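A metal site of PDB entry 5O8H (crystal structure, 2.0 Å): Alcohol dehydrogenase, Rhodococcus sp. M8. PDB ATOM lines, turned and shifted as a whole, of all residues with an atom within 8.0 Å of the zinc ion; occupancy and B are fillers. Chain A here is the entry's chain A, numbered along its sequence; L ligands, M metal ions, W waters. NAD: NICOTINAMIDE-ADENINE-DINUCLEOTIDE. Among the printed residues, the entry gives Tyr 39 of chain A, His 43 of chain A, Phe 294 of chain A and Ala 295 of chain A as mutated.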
ATOM      1  N   GLY A  36       5.345 -11.804  21.945  1.00  0.00           N
ATOM      2  CA  GLY A  36       4.372 -10.885  22.514  1.00  0.00           C
ATOM      3  C   GLY A  36       2.934 -11.370  22.342  1.00  0.00           C
ATOM      4  O   GLY A  36       2.609 -12.021  21.354  1.00  0.00           O
ATOM      5  N   LEU A  37       2.092 -11.066  23.325  1.00  0.00           N
ATOM      6  CA  LEU A  37       0.650 -11.302  23.231  1.00  0.00           C
ATOM      7  C   LEU A  37      -0.012 -10.006  22.808  1.00  0.00           C
ATOM      8  O   LEU A  37       0.184  -8.985  23.479  1.00  0.00           O
ATOM      9  CB  LEU A  37       0.064 -11.687  24.586  1.00  0.00           C
ATOM     10  CG  LEU A  37       0.227 -13.096  25.126  1.00  0.00           C
ATOM     11  CD1 LEU A  37       1.632 -13.310  25.639  1.00  0.00           C
ATOM     12  CD2 LEU A  37      -0.770 -13.317  26.250  1.00  0.00           C
ATOM     13  N   CYS A  38      -0.797 -10.039  21.731  1.00  0.00           N
ATOM     14  CA  CYS A  38      -1.521  -8.839  21.264  1.00  0.00           C
ATOM     15  C   CYS A  38      -3.019  -9.087  21.385  1.00  0.00           C
ATOM     16  O   CYS A  38      -3.503 -10.203  21.147  1.00  0.00           O
ATOM     17  CB  CYS A  38      -1.203  -8.535  19.815  1.00  0.00           C
ATOM     18  SG  CYS A  38      -2.051  -7.012  19.242  1.00  0.00           S
ATOM     19  N   TYR A  39      -3.763  -8.025  21.712  1.00  0.00           N
ATOM     20  CA  TYR A  39      -5.202  -8.163  21.879  1.00  0.00           C
ATOM     21  C   TYR A  39      -5.887  -8.607  20.580  1.00  0.00           C
ATOM     22  O   TYR A  39      -6.973  -9.189  20.605  1.00  0.00           O
ATOM     23  CB  TYR A  39      -5.840  -6.891  22.474  1.00  0.00           C
ATOM     24  CG  TYR A  39      -7.202  -7.150  23.057  1.00  0.00           C
ATOM     25  CD1 TYR A  39      -8.339  -7.078  22.255  1.00  0.00           C
ATOM     26  CD2 TYR A  39      -7.368  -7.504  24.389  1.00  0.00           C
ATOM     27  CE1 TYR A  39      -9.603  -7.327  22.788  1.00  0.00           C
ATOM     28  CE2 TYR A  39      -8.624  -7.773  24.909  1.00  0.00           C
ATOM     29  CZ  TYR A  39      -9.740  -7.682  24.083  1.00  0.00           C
ATOM     30  OH  TYR A  39     -11.002  -7.925  24.555  1.00  0.00           O
ATOM     31  N   SER A  40      -5.229  -8.382  19.435  1.00  0.00           N
ATOM     32  CA  SER A  40      -5.704  -8.932  18.167  1.00  0.00           C
ATOM     33  C   SER A  40      -5.857 -10.462  18.202  1.00  0.00           C
ATOM     34  O   SER A  40      -6.739 -11.001  17.531  1.00  0.00           O
ATOM     35  CB  SER A  40      -4.799  -8.519  17.003  1.00  0.00           C
ATOM     36  OG  SER A  40      -4.942  -7.111  16.746  1.00  0.00           O
ATOM     37  N   ASP A  41      -5.011 -11.160  18.973  1.00  0.00           N
ATOM     38  CA  ASP A  41      -5.133 -12.613  19.149  1.00  0.00           C
ATOM     39  C   ASP A  41      -6.494 -13.005  19.785  1.00  0.00           C
ATOM     40  O   ASP A  41      -7.059 -14.043  19.446  1.00  0.00           O
ATOM     41  CB  ASP A  41      -4.012 -13.144  20.027  1.00  0.00           C
ATOM     42  CG  ASP A  41      -2.627 -12.917  19.427  1.00  0.00           C
ATOM     43  OD1 ASP A  41      -2.535 -12.865  18.173  1.00  0.00           O
ATOM     44  OD2 ASP A  41      -1.628 -12.824  20.197  1.00  0.00           O
ATOM     45  N   HIS A  43      -9.311 -11.063  19.403  1.00  0.00           N
ATOM     46  CA  HIS A  43     -10.278 -10.871  18.296  1.00  0.00           C
ATOM     47  C   HIS A  43     -10.334 -12.154  17.457  1.00  0.00           C
ATOM     48  O   HIS A  43     -11.418 -12.643  17.159  1.00  0.00           O
ATOM     49  CB  HIS A  43      -9.949  -9.670  17.385  1.00  0.00           C
ATOM     50  CG  HIS A  43     -10.008  -8.338  18.078  1.00  0.00           C
ATOM     51  ND1 HIS A  43     -11.028  -7.964  18.918  1.00  0.00           N
ATOM     52  CD2 HIS A  43      -9.152  -7.280  18.030  1.00  0.00           C
ATOM     53  CE1 HIS A  43     -10.809  -6.741  19.362  1.00  0.00           C
ATOM     54  NE2 HIS A  43      -9.679  -6.301  18.838  1.00  0.00           N
ATOM     55  N   GLY A  61       1.010 -15.995  18.101  1.00  0.00           N
ATOM     56  CA  GLY A  61       2.119 -15.076  18.350  1.00  0.00           C
ATOM     57  C   GLY A  61       2.569 -14.365  17.084  1.00  0.00           C
ATOM     58  O   GLY A  61       3.328 -14.940  16.295  1.00  0.00           O
ATOM     59  N   HIS A  62       2.119 -13.122  16.891  1.00  0.00           N
ATOM     60  CA  HIS A  62       2.569 -12.312  15.724  1.00  0.00           C
ATOM     61  C   HIS A  62       3.609 -11.269  16.077  1.00  0.00           C
ATOM     62  O   HIS A  62       4.082 -10.552  15.186  1.00  0.00           O
ATOM     63  CB  HIS A  62       1.430 -11.701  14.885  1.00  0.00           C
ATOM     64  CG  HIS A  62       0.406 -10.963  15.658  1.00  0.00           C
ATOM     65  ND1 HIS A  62      -0.753 -11.551  16.117  1.00  0.00           N
ATOM     66  CD2 HIS A  62       0.336  -9.668  16.023  1.00  0.00           C
ATOM     67  CE1 HIS A  62      -1.503 -10.636  16.711  1.00  0.00           C
ATOM     68  NE2 HIS A  62      -0.849  -9.498  16.690  1.00  0.00           N
ATOM     69  N   GLU A  63       4.001 -11.222  17.350  1.00  0.00           N
ATOM     70  CA  GLU A  63       5.145 -10.434  17.828  1.00  0.00           C
ATOM     71  C   GLU A  63       6.261 -11.400  18.199  1.00  0.00           C
ATOM     72  O   GLU A  63       6.171 -12.094  19.206  1.00  0.00           O
ATOM     73  CB  GLU A  63       4.752  -9.583  19.040  1.00  0.00           C
ATOM     74  CG  GLU A  63       3.781  -8.447  18.712  1.00  0.00           C
ATOM     75  CD  GLU A  63       3.444  -7.550  19.905  1.00  0.00           C
ATOM     76  OE1 GLU A  63       3.708  -7.932  21.074  1.00  0.00           O
ATOM     77  OE2 GLU A  63       2.885  -6.453  19.684  1.00  0.00           O
ATOM     78  N   LEU A 119      -1.162 -15.641  12.404  1.00  0.00           N
ATOM     79  CA  LEU A 119      -2.442 -15.213  11.828  1.00  0.00           C
ATOM     80  C   LEU A 119      -2.625 -15.869  10.452  1.00  0.00           C
ATOM     81  O   LEU A 119      -3.031 -15.223   9.484  1.00  0.00           O
ATOM     82  CB  LEU A 119      -2.487 -13.665  11.724  1.00  0.00           C
ATOM     83  CG  LEU A 119      -2.267 -12.831  13.001  1.00  0.00           C
ATOM     84  CD1 LEU A 119      -2.015 -11.361  12.728  1.00  0.00           C
ATOM     85  CD2 LEU A 119      -3.438 -12.973  13.963  1.00  0.00           C
ATOM     86  N   THR A 152       7.615  -5.183  17.421  1.00  0.00           N
ATOM     87  CA  THR A 152       7.170  -5.707  16.139  1.00  0.00           C
ATOM     88  C   THR A 152       5.673  -5.466  15.842  1.00  0.00           C
ATOM     89  O   THR A 152       5.237  -5.681  14.711  1.00  0.00           O
ATOM     90  CB  THR A 152       7.445  -7.223  16.034  1.00  0.00           C
ATOM     91  OG1 THR A 152       6.743  -7.943  17.054  1.00  0.00           O
ATOM     92  CG2 THR A 152       8.923  -7.516  16.168  1.00  0.00           C
ATOM     93  N   ASP A 153       4.893  -5.070  16.838  1.00  0.00           N
ATOM     94  CA  ASP A 153       3.512  -4.675  16.568  1.00  0.00           C
ATOM     95  C   ASP A 153       3.006  -3.551  17.473  1.00  0.00           C
ATOM     96  O   ASP A 153       2.534  -2.520  16.984  1.00  0.00           O
ATOM     97  CB  ASP A 153       2.599  -5.894  16.586  1.00  0.00           C
ATOM     98  CG  ASP A 153       1.300  -5.682  15.837  1.00  0.00           C
ATOM     99  OD1 ASP A 153       1.179  -4.846  14.893  1.00  0.00           O
ATOM    100  OD2 ASP A 153       0.396  -6.422  16.192  1.00  0.00           O
ATOM    101  N   ALA A 154       3.128  -3.735  18.797  1.00  0.00           N
ATOM    102  CA  ALA A 154       2.845  -2.665  19.724  1.00  0.00           C
ATOM    103  C   ALA A 154       3.672  -1.405  19.450  1.00  0.00           C
ATOM    104  O   ALA A 154       3.193  -0.325  19.692  1.00  0.00           O
ATOM    105  CB  ALA A 154       3.046  -3.137  21.177  1.00  0.00           C
ATOM    106  N   THR A 157       2.882  -0.587  14.878  1.00  0.00           N
ATOM    107  CA  THR A 157       1.584  -0.091  14.474  1.00  0.00           C
ATOM    108  C   THR A 157       1.353   1.392  14.854  1.00  0.00           C
ATOM    109  O   THR A 157       0.987   2.193  13.969  1.00  0.00           O
ATOM    110  CB  THR A 157       0.453  -1.027  14.945  1.00  0.00           C
ATOM    111  OG1 THR A 157       0.597  -2.270  14.261  1.00  0.00           O
ATOM    112  CG2 THR A 157      -0.896  -0.459  14.628  1.00  0.00           C
ATOM    113  N   LEU A 183      -0.243  -1.049  22.836  1.00  0.00           N
ATOM    114  CA  LEU A 183       0.038  -0.089  21.766  1.00  0.00           C
ATOM    115  C   LEU A 183       0.174   1.330  22.301  1.00  0.00           C
ATOM    116  O   LEU A 183       1.174   2.018  22.025  1.00  0.00           O
ATOM    117  CB  LEU A 183      -1.026  -0.116  20.645  1.00  0.00           C
ATOM    118  CG  LEU A 183      -0.776  -1.091  19.506  1.00  0.00           C
ATOM    119  CD1 LEU A 183      -0.862  -2.548  19.930  1.00  0.00           C
ATOM    120  CD2 LEU A 183      -1.717  -0.836  18.357  1.00  0.00           C
ATOM    121  N   ILE A 271      -9.525  -1.907  17.097  1.00  0.00           N
ATOM    122  CA  ILE A 271     -10.530  -2.637  16.327  1.00  0.00           C
ATOM    123  C   ILE A 271     -11.701  -3.010  17.242  1.00  0.00           C
ATOM    124  O   ILE A 271     -11.522  -3.695  18.255  1.00  0.00           O
ATOM    125  CB  ILE A 271      -9.920  -3.916  15.697  1.00  0.00           C
ATOM    126  CG1 ILE A 271      -8.743  -3.549  14.770  1.00  0.00           C
ATOM    127  CG2 ILE A 271     -10.976  -4.709  14.923  1.00  0.00           C
ATOM    128  CD1 ILE A 271      -7.830  -4.716  14.422  1.00  0.00           C
ATOM    129  N   PHE A 294      -2.911   0.106   9.097  1.00  0.00           N
ATOM    130  CA  PHE A 294      -2.641  -1.322   9.357  1.00  0.00           C
ATOM    131  C   PHE A 294      -1.141  -1.573   9.448  1.00  0.00           C
ATOM    132  O   PHE A 294      -0.404  -1.301   8.514  1.00  0.00           O
ATOM    133  CB  PHE A 294      -3.204  -2.229   8.279  1.00  0.00           C
ATOM    134  CG  PHE A 294      -2.976  -3.700   8.555  1.00  0.00           C
ATOM    135  CD1 PHE A 294      -3.607  -4.330   9.628  1.00  0.00           C
ATOM    136  CD2 PHE A 294      -2.140  -4.449   7.739  1.00  0.00           C
ATOM    137  CE1 PHE A 294      -3.374  -5.691   9.890  1.00  0.00           C
ATOM    138  CE2 PHE A 294      -1.920  -5.803   7.983  1.00  0.00           C
ATOM    139  CZ  PHE A 294      -2.531  -6.423   9.053  1.00  0.00           C
ATOM    140  N   ALA A 295      -0.725  -2.071  10.609  1.00  0.00           N
ATOM    141  CA  ALA A 295       0.618  -2.527  10.862  1.00  0.00           C
ATOM    142  C   ALA A 295       1.631  -1.429  10.498  1.00  0.00           C
ATOM    143  O   ALA A 295       1.411  -0.295  10.873  1.00  0.00           O
ATOM    144  CB  ALA A 295       0.870  -3.855  10.150  1.00  0.00           C
ATOM    145  N   ARG A 340       2.541  -4.854  27.976  1.00  0.00           N
ATOM    146  CA  ARG A 340       2.532  -6.012  27.094  1.00  0.00           C
ATOM    147  C   ARG A 340       2.914  -7.309  27.789  1.00  0.00           C
ATOM    148  O   ARG A 340       3.935  -7.368  28.453  1.00  0.00           O
ATOM    149  CB  ARG A 340       3.540  -5.802  25.946  1.00  0.00           C
ATOM    150  CG  ARG A 340       2.876  -5.507  24.640  1.00  0.00           C
ATOM    151  CD  ARG A 340       2.289  -6.753  24.046  1.00  0.00           C
ATOM    152  NE  ARG A 340       1.870  -6.500  22.666  1.00  0.00           N
ATOM    153  CZ  ARG A 340       0.702  -5.976  22.277  1.00  0.00           C
ATOM    154  NH1 ARG A 340      -0.242  -5.617  23.152  1.00  0.00           N
ATOM    155  NH2 ARG A 340       0.496  -5.826  20.979  1.00  0.00           N
HETATM  156  PA  NAD L   1      -4.564  -3.812  25.387  1.00  0.00           P
HETATM  157  O1A NAD L   1      -5.648  -4.622  25.959  1.00  0.00           O
HETATM  158  O2A NAD L   1      -3.128  -3.997  25.783  1.00  0.00           O
HETATM  159  O5B NAD L   1      -4.875  -2.277  25.798  1.00  0.00           O
HETATM  160  C5B NAD L   1      -6.182  -1.755  25.879  1.00  0.00           C
HETATM  161  C4B NAD L   1      -6.138  -0.412  26.591  1.00  0.00           C
HETATM  162  O4B NAD L   1      -7.274   0.325  26.180  1.00  0.00           O
HETATM  163  C3B NAD L   1      -6.224  -0.546  28.115  1.00  0.00           C
HETATM  164  O3B NAD L   1      -5.318   0.349  28.753  1.00  0.00           O
HETATM  165  C2B NAD L   1      -7.678  -0.218  28.419  1.00  0.00           C
HETATM  166  O2B NAD L   1      -7.917   0.323  29.711  1.00  0.00           O
HETATM  167  C1B NAD L   1      -7.955   0.812  27.336  1.00  0.00           C
HETATM  168  N9A NAD L   1      -9.404   0.989  27.014  1.00  0.00           N
HETATM  169  C8A NAD L   1     -10.339   0.050  26.748  1.00  0.00           C
HETATM  170  N7A NAD L   1     -11.526   0.639  26.491  1.00  0.00           N
HETATM  171  C5A NAD L   1     -11.342   1.969  26.581  1.00  0.00           C
HETATM  172  C6A NAD L   1     -12.153   3.174  26.408  1.00  0.00           C
HETATM  173  N6A NAD L   1     -13.456   3.090  26.091  1.00  0.00           N
HETATM  174  N1A NAD L   1     -11.581   4.379  26.573  1.00  0.00           N
HETATM  175  C2A NAD L   1     -10.265   4.493  26.900  1.00  0.00           C
HETATM  176  N3A NAD L   1      -9.449   3.436  27.091  1.00  0.00           N
HETATM  177  C4A NAD L   1      -9.936   2.192  26.927  1.00  0.00           C
HETATM  178  O3  NAD L   1      -4.762  -3.798  23.781  1.00  0.00           O
HETATM  179  PN  NAD L   1      -3.568  -3.549  22.679  1.00  0.00           P
HETATM  180  O1N NAD L   1      -2.845  -4.823  22.466  1.00  0.00           O
HETATM  181  O2N NAD L   1      -2.868  -2.260  23.027  1.00  0.00           O
HETATM  182  O5D NAD L   1      -4.519  -3.411  21.392  1.00  0.00           O
HETATM  183  C5D NAD L   1      -5.379  -2.266  21.267  1.00  0.00           C
HETATM  184  C4D NAD L   1      -6.199  -2.414  20.005  1.00  0.00           C
HETATM  185  O4D NAD L   1      -5.336  -2.244  18.864  1.00  0.00           O
HETATM  186  C3D NAD L   1      -6.890  -3.782  19.824  1.00  0.00           C
HETATM  187  O3D NAD L   1      -8.240  -3.603  19.380  1.00  0.00           O
HETATM  188  C2D NAD L   1      -6.048  -4.458  18.766  1.00  0.00           C
HETATM  189  O2D NAD L   1      -6.751  -5.478  18.037  1.00  0.00           O
HETATM  190  C1D NAD L   1      -5.670  -3.236  17.927  1.00  0.00           C
HETATM  191  N1N NAD L   1      -4.525  -3.397  17.024  1.00  0.00           N
HETATM  192  C2N NAD L   1      -4.646  -2.892  15.782  1.00  0.00           C
HETATM  193  C3N NAD L   1      -3.614  -2.993  14.865  1.00  0.00           C
HETATM  194  C7N NAD L   1      -3.720  -2.410  13.492  1.00  0.00           C
HETATM  195  O7N NAD L   1      -2.930  -2.762  12.650  1.00  0.00           O
HETATM  196  N7N NAD L   1      -4.625  -1.458  13.220  1.00  0.00           N
HETATM  197  C4N NAD L   1      -2.415  -3.642  15.248  1.00  0.00           C
HETATM  198  C5N NAD L   1      -2.317  -4.136  16.567  1.00  0.00           C
HETATM  199  C6N NAD L   1      -3.372  -3.996  17.431  1.00  0.00           C
HETATM  200 ZN    ZN M   1      -1.319  -7.485  16.745  1.00  0.00          ZN
HETATM  201  O   HOH W   1      -2.358  -7.566  14.428  1.00  0.00           O
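Residues that only touch the zinc ion: Ser 40 (3.6 Å). Of the 20 residues printed, 4 come within 4 Å of the zinc ion.
The zinc ion is bound by NE2 of His 62 (2.1 Å), OD2 of Asp 153 (2.1 Å), water W1 (2.5 Å) and SG of Cys 38 (2.6 Å). The zinc ion has four donor atoms within binding distance.
OG of Ser 40 lies within hydrogen-bond range of O2D of the ligand, 2.8 Å away. The guanidinium group of Arg 340 lies within salt-bridge range of an oxygen (O1N) of the ligand, 2.8 Å away. An oxygen (O1N) of the ligand sits at hydrogen-bond distance from the backbone NH (N) of Tyr 39 (3.4 Å). The backbone NH of Leu 183 sits at hydrogen-bond distance from an oxygen (O2N) of the ligand (2.9 Å). N of Ile 271 is in hydrogen-bond range of O3D of the ligand (3.1 Å). An oxygen (O3D) of the ligand sits at hydrogen-bond distance from the backbone carbonyl oxygen (O) of Ile 271 (3.5 Å). N of Ala 295 sits at hydrogen-bond distance from O7N of the ligand (3.1 Å). A ring nitrogen (NE2) of His 43 sits at hydrogen-bond distance from an oxygen (O3D) of the ligand, at 3.1 Å.
The side-chain carboxylate of Asp 41 sits close to a ring nitrogen (ND1) of His 62, 3.0 Å away. OD1 of Asp 153 sits at hydrogen-bond distance from OG1 of Thr 157, at 2.7 Å. The side-chain sulfur (SG) of Cys 38 sits close to the backbone NH (N) of Ser 40. The guanidinium group of Arg 340 sits close to the side-chain sulfur of Cys 38, 3.3 Å away. OD2 of Asp 41 lies within hydrogen-bond range of N of Cys 38, 3.3 Å away.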
